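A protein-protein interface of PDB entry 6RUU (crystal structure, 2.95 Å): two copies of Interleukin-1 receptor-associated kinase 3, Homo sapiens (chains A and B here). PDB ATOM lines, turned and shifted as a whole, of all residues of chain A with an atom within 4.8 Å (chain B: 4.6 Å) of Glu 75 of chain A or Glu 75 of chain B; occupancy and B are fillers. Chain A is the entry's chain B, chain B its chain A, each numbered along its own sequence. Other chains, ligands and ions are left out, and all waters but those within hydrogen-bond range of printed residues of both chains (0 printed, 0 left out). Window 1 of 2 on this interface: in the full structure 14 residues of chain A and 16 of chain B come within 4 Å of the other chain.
Glu 75 of chain A touches just these residues of chain B: Leu 71 (3.2 Å) and Glu 75 (2.6 Å). Glu 75 of chain B touches two residues of chain A. Of the printed residues of chain A, Leu 79 of chain B touches Leu 71 (3.7 Å). Of the printed residues of chain A, Leu 78 of chain B touches Leu 78. Printed residues of chain B within 4 Å of Leu 78 of chain A: Leu 78. Of the printed residues of chain A, Phe 178 of chain B touches Leu 71.
Hydrophobic or aromatic side chains of chain A that line the printed part of chain B: Leu 71, Leu 78 and Leu 79. Among the printed residues, 7 pairs touch across the chains.
The side-chain carboxylate (OE2) of Glu 75 of chain A lies close to the side-chain carboxylate (OE2) of Glu 75 of chain B.
Leu 71 of chain A touches Glu 75 of chain B, and with the chains exchanged Glu 75 of chain A touches Leu 71 of chain B. Leu 71 of chain A touches Leu 79 of chain B, but with the chains exchanged Leu 79 of chain A does not touch Leu 71 of chain B (5.0 Å). Leu 71 of chain A touches Phe 178 of chain B, but with the chains exchanged Phe 178 of chain A does not touch Leu 71 of chain B (4.1 Å). Glu 75 of chain B touches its own counterpart, Glu 75 of chain A. Positions printed for both chains: 71, 72, 73, 74, 75, 76, 77, 78, 79 and 178. Of the 7 pairs that touch across the chains among the printed residues, 4 have their exchanged pair printed and touching as well.
Among the printed residues, pairs that only touch across the chains: Leu 71 of chain A with Glu 75 of chain B (3.3 Å), Leu 71 of chain A with Leu 79 of chain B (3.7 Å), Leu 71 of chain A with Phe 178 of chain B (3.8 Å), Glu 75 of chain A with Leu 71 of chain B (3.2 Å), Leu 78 of chain A with Leu 78 of chain B (3.9 Å) and Leu 79 of chain A with Leu 74 of chain B (3.6 Å).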
ATOM      1  N   LEU A  71       8.107  26.052  29.152  1.00  0.00           N
ATOM      2  CA  LEU A  71       7.796  26.757  27.916  1.00  0.00           C
ATOM      3  C   LEU A  71       6.748  27.836  28.158  1.00  0.00           C
ATOM      4  O   LEU A  71       7.011  29.027  27.956  1.00  0.00           O
ATOM      5  CB  LEU A  71       7.327  25.765  26.850  1.00  0.00           C
ATOM      6  CG  LEU A  71       8.375  24.758  26.368  1.00  0.00           C
ATOM      7  CD1 LEU A  71       7.765  23.764  25.390  1.00  0.00           C
ATOM      8  CD2 LEU A  71       9.571  25.462  25.747  1.00  0.00           C
ATOM      9  N   SER A  72       5.557  27.434  28.619  1.00  0.00           N
ATOM     10  CA  SER A  72       4.460  28.380  28.819  1.00  0.00           C
ATOM     11  C   SER A  72       4.896  29.580  29.645  1.00  0.00           C
ATOM     12  O   SER A  72       4.460  30.709  29.393  1.00  0.00           O
ATOM     13  CB  SER A  72       3.275  27.681  29.485  1.00  0.00           C
ATOM     14  OG  SER A  72       2.725  26.691  28.637  1.00  0.00           O
ATOM     15  N   GLU A  73       5.762  29.355  30.634  1.00  0.00           N
ATOM     16  CA  GLU A  73       6.323  30.460  31.406  1.00  0.00           C
ATOM     17  C   GLU A  73       7.075  31.429  30.501  1.00  0.00           C
ATOM     18  O   GLU A  73       6.781  32.629  30.466  1.00  0.00           O
ATOM     19  CB  GLU A  73       7.243  29.909  32.497  1.00  0.00           C
ATOM     20  CG  GLU A  73       7.868  30.964  33.396  1.00  0.00           C
ATOM     21  CD  GLU A  73       6.852  31.669  34.271  1.00  0.00           C
ATOM     22  OE1 GLU A  73       5.788  31.076  34.548  1.00  0.00           O
ATOM     23  OE2 GLU A  73       7.122  32.813  34.692  1.00  0.00           O
ATOM     24  N   LEU A  74       8.046  30.914  29.743  1.00  0.00           N
ATOM     25  CA  LEU A  74       8.867  31.772  28.896  1.00  0.00           C
ATOM     26  C   LEU A  74       8.080  32.310  27.706  1.00  0.00           C
ATOM     27  O   LEU A  74       8.419  33.371  27.170  1.00  0.00           O
ATOM     28  CB  LEU A  74      10.103  30.997  28.433  1.00  0.00           C
ATOM     29  CG  LEU A  74      11.260  31.710  27.730  1.00  0.00           C
ATOM     30  CD1 LEU A  74      12.561  30.977  28.012  1.00  0.00           C
ATOM     31  CD2 LEU A  74      11.029  31.788  26.234  1.00  0.00           C
ATOM     32  N   GLU A  75       7.040  31.596  27.276  1.00  0.00           N
ATOM     33  CA  GLU A  75       6.205  32.068  26.175  1.00  0.00           C
ATOM     34  C   GLU A  75       5.554  33.402  26.518  1.00  0.00           C
ATOM     35  O   GLU A  75       5.735  34.402  25.816  1.00  0.00           O
ATOM     36  CB  GLU A  75       5.130  31.030  25.862  1.00  0.00           C
ATOM     37  CG  GLU A  75       5.635  29.703  25.346  1.00  0.00           C
ATOM     38  CD  GLU A  75       4.533  28.666  25.322  1.00  0.00           C
ATOM     39  OE1 GLU A  75       3.417  28.976  25.788  1.00  0.00           O
ATOM     40  OE2 GLU A  75       4.773  27.539  24.850  1.00  0.00           O
ATOM     41  N   VAL A  76       4.789  33.428  27.611  1.00  0.00           N
ATOM     42  CA  VAL A  76       3.973  34.595  27.930  1.00  0.00           C
ATOM     43  C   VAL A  76       4.850  35.789  28.289  1.00  0.00           C
ATOM     44  O   VAL A  76       4.536  36.933  27.939  1.00  0.00           O
ATOM     45  CB  VAL A  76       2.986  34.251  29.061  1.00  0.00           C
ATOM     46  CG1 VAL A  76       2.164  35.470  29.455  1.00  0.00           C
ATOM     47  CG2 VAL A  76       2.083  33.100  28.642  1.00  0.00           C
ATOM     48  N   LEU A  77       5.966  35.546  28.979  1.00  0.00           N
ATOM     49  CA  LEU A  77       6.792  36.654  29.453  1.00  0.00           C
ATOM     50  C   LEU A  77       7.469  37.383  28.299  1.00  0.00           C
ATOM     51  O   LEU A  77       7.575  38.615  28.314  1.00  0.00           O
ATOM     52  CB  LEU A  77       7.830  36.143  30.448  1.00  0.00           C
ATOM     53  CG  LEU A  77       7.283  35.630  31.780  1.00  0.00           C
ATOM     54  CD1 LEU A  77       8.401  35.038  32.611  1.00  0.00           C
ATOM     55  CD2 LEU A  77       6.587  36.745  32.540  1.00  0.00           C
ATOM     56  N   LEU A  78       7.932  36.644  27.292  1.00  0.00           N
ATOM     57  CA  LEU A  78       8.582  37.274  26.148  1.00  0.00           C
ATOM     58  C   LEU A  78       7.585  37.956  25.220  1.00  0.00           C
ATOM     59  O   LEU A  78       7.899  39.005  24.645  1.00  0.00           O
ATOM     60  CB  LEU A  78       9.404  36.242  25.374  1.00  0.00           C
ATOM     61  CG  LEU A  78      10.833  35.991  25.859  1.00  0.00           C
ATOM     62  CD1 LEU A  78      10.872  35.337  27.227  1.00  0.00           C
ATOM     63  CD2 LEU A  78      11.579  35.134  24.853  1.00  0.00           C
ATOM     64  N   LEU A  79       6.388  37.398  25.071  1.00  0.00           N
ATOM     65  CA  LEU A  79       5.425  37.915  24.108  1.00  0.00           C
ATOM     66  C   LEU A  79       4.486  38.965  24.684  1.00  0.00           C
ATOM     67  O   LEU A  79       3.921  39.753  23.917  1.00  0.00           O
ATOM     68  CB  LEU A  79       4.589  36.772  23.521  1.00  0.00           C
ATOM     69  CG  LEU A  79       5.203  35.988  22.359  1.00  0.00           C
ATOM     70  CD1 LEU A  79       6.362  35.125  22.819  1.00  0.00           C
ATOM     71  CD2 LEU A  79       4.143  35.141  21.672  1.00  0.00           C
ATOM     72  N   PHE A 178      -3.871  29.423  26.057  1.00  0.00           N
ATOM     73  CA  PHE A 178      -4.497  30.281  25.062  1.00  0.00           C
ATOM     74  C   PHE A 178      -5.852  29.693  24.686  1.00  0.00           C
ATOM     75  O   PHE A 178      -6.008  28.471  24.613  1.00  0.00           O
ATOM     76  CB  PHE A 178      -3.597  30.394  23.833  1.00  0.00           C
ATOM     77  CG  PHE A 178      -2.246  30.988  24.126  1.00  0.00           C
ATOM     78  CD1 PHE A 178      -2.047  32.358  24.089  1.00  0.00           C
ATOM     79  CD2 PHE A 178      -1.182  30.172  24.478  1.00  0.00           C
ATOM     80  CE1 PHE A 178      -0.801  32.900  24.367  1.00  0.00           C
ATOM     81  CE2 PHE A 178       0.061  30.709  24.763  1.00  0.00           C
ATOM     82  CZ  PHE A 178       0.252  32.072  24.705  1.00  0.00           C
ATOM     83  N   LEU B  71       4.393  29.130  18.105  1.00  0.00           N
ATOM     84  CA  LEU B  71       5.234  28.917  19.277  1.00  0.00           C
ATOM     85  C   LEU B  71       6.299  27.859  19.020  1.00  0.00           C
ATOM     86  O   LEU B  71       7.417  27.972  19.535  1.00  0.00           O
ATOM     87  CB  LEU B  71       4.366  28.531  20.475  1.00  0.00           C
ATOM     88  CG  LEU B  71       3.751  29.672  21.292  1.00  0.00           C
ATOM     89  CD1 LEU B  71       2.764  30.492  20.489  1.00  0.00           C
ATOM     90  CD2 LEU B  71       3.046  29.099  22.496  1.00  0.00           C
ATOM     91  N   SER B  72       5.980  26.833  18.229  1.00  0.00           N
ATOM     92  CA  SER B  72       6.965  25.795  17.933  1.00  0.00           C
ATOM     93  C   SER B  72       8.215  26.391  17.298  1.00  0.00           C
ATOM     94  O   SER B  72       9.340  26.097  17.722  1.00  0.00           O
ATOM     95  CB  SER B  72       6.352  24.728  17.026  1.00  0.00           C
ATOM     96  OG  SER B  72       5.304  24.039  17.686  1.00  0.00           O
ATOM     97  N   GLU B  73       8.036  27.234  16.277  1.00  0.00           N
ATOM     98  CA  GLU B  73       9.147  27.989  15.704  1.00  0.00           C
ATOM     99  C   GLU B  73       9.968  28.674  16.785  1.00  0.00           C
ATOM    100  O   GLU B  73      11.170  28.428  16.929  1.00  0.00           O
ATOM    101  CB  GLU B  73       8.621  29.034  14.716  1.00  0.00           C
ATOM    102  CG  GLU B  73       8.284  28.530  13.333  1.00  0.00           C
ATOM    103  CD  GLU B  73       9.526  28.272  12.507  1.00  0.00           C
ATOM    104  OE1 GLU B  73      10.547  28.953  12.736  1.00  0.00           O
ATOM    105  OE2 GLU B  73       9.477  27.407  11.614  1.00  0.00           O
ATOM    106  N   LEU B  74       9.318  29.539  17.562  1.00  0.00           N
ATOM    107  CA  LEU B  74      10.043  30.410  18.475  1.00  0.00           C
ATOM    108  C   LEU B  74      10.724  29.617  19.582  1.00  0.00           C
ATOM    109  O   LEU B  74      11.846  29.945  19.984  1.00  0.00           O
ATOM    110  CB  LEU B  74       9.087  31.448  19.060  1.00  0.00           C
ATOM    111  CG  LEU B  74       9.703  32.518  19.953  1.00  0.00           C
ATOM    112  CD1 LEU B  74      10.683  33.345  19.154  1.00  0.00           C
ATOM    113  CD2 LEU B  74       8.612  33.392  20.529  1.00  0.00           C
ATOM    114  N   GLU B  75      10.069  28.567  20.077  1.00  0.00           N
ATOM    115  CA  GLU B  75      10.643  27.773  21.156  1.00  0.00           C
ATOM    116  C   GLU B  75      11.975  27.161  20.741  1.00  0.00           C
ATOM    117  O   GLU B  75      13.012  27.410  21.365  1.00  0.00           O
ATOM    118  CB  GLU B  75       9.665  26.678  21.582  1.00  0.00           C
ATOM    119  CG  GLU B  75       8.456  27.165  22.357  1.00  0.00           C
ATOM    120  CD  GLU B  75       7.506  26.033  22.684  1.00  0.00           C
ATOM    121  OE1 GLU B  75       7.700  24.921  22.150  1.00  0.00           O
ATOM    122  OE2 GLU B  75       6.579  26.243  23.485  1.00  0.00           O
ATOM    123  N   VAL B  76      11.965  26.360  19.674  1.00  0.00           N
ATOM    124  CA  VAL B  76      13.153  25.591  19.326  1.00  0.00           C
ATOM    125  C   VAL B  76      14.274  26.500  18.835  1.00  0.00           C
ATOM    126  O   VAL B  76      15.456  26.195  19.028  1.00  0.00           O
ATOM    127  CB  VAL B  76      12.795  24.504  18.293  1.00  0.00           C
ATOM    128  CG1 VAL B  76      12.372  25.135  16.994  1.00  0.00           C
ATOM    129  CG2 VAL B  76      13.961  23.557  18.075  1.00  0.00           C
ATOM    130  N   LEU B  77      13.935  27.635  18.219  1.00  0.00           N
ATOM    131  CA  LEU B  77      14.965  28.538  17.722  1.00  0.00           C
ATOM    132  C   LEU B  77      15.647  29.322  18.833  1.00  0.00           C
ATOM    133  O   LEU B  77      16.778  29.784  18.642  1.00  0.00           O
ATOM    134  CB  LEU B  77      14.377  29.507  16.696  1.00  0.00           C
ATOM    135  CG  LEU B  77      13.946  28.887  15.369  1.00  0.00           C
ATOM    136  CD1 LEU B  77      13.264  29.925  14.496  1.00  0.00           C
ATOM    137  CD2 LEU B  77      15.146  28.286  14.658  1.00  0.00           C
ATOM    138  N   LEU B  78      14.993  29.484  19.981  1.00  0.00           N
ATOM    139  CA  LEU B  78      15.600  30.176  21.110  1.00  0.00           C
ATOM    140  C   LEU B  78      16.313  29.229  22.061  1.00  0.00           C
ATOM    141  O   LEU B  78      17.250  29.643  22.752  1.00  0.00           O
ATOM    142  CB  LEU B  78      14.539  30.955  21.889  1.00  0.00           C
ATOM    143  CG  LEU B  78      13.856  32.116  21.174  1.00  0.00           C
ATOM    144  CD1 LEU B  78      12.752  32.674  22.051  1.00  0.00           C
ATOM    145  CD2 LEU B  78      14.864  33.191  20.806  1.00  0.00           C
ATOM    146  N   LEU B  79      15.890  27.971  22.113  1.00  0.00           N
ATOM    147  CA  LEU B  79      16.443  27.016  23.058  1.00  0.00           C
ATOM    148  C   LEU B  79      17.538  26.149  22.463  1.00  0.00           C
ATOM    149  O   LEU B  79      18.326  25.571  23.220  1.00  0.00           O
ATOM    150  CB  LEU B  79      15.332  26.107  23.597  1.00  0.00           C
ATOM    151  CG  LEU B  79      14.200  26.811  24.345  1.00  0.00           C
ATOM    152  CD1 LEU B  79      13.097  25.832  24.678  1.00  0.00           C
ATOM    153  CD2 LEU B  79      14.712  27.488  25.599  1.00  0.00           C
ATOM    154  N   PHE B 178       7.870  17.775  21.073  1.00  0.00           N
ATOM    155  CA  PHE B 178       8.794  17.343  22.113  1.00  0.00           C
ATOM    156  C   PHE B 178       8.363  15.968  22.612  1.00  0.00           C
ATOM    157  O   PHE B 178       7.240  15.807  23.101  1.00  0.00           O
ATOM    158  CB  PHE B 178       8.819  18.345  23.266  1.00  0.00           C
ATOM    159  CG  PHE B 178       9.316  19.708  22.877  1.00  0.00           C
ATOM    160  CD1 PHE B 178      10.673  19.969  22.783  1.00  0.00           C
ATOM    161  CD2 PHE B 178       8.420  20.730  22.604  1.00  0.00           C
ATOM    162  CE1 PHE B 178      11.127  21.227  22.427  1.00  0.00           C
ATOM    163  CE2 PHE B 178       8.868  21.988  22.247  1.00  0.00           C
ATOM    164  CZ  PHE B 178      10.223  22.237  22.158  1.00  0.00           C
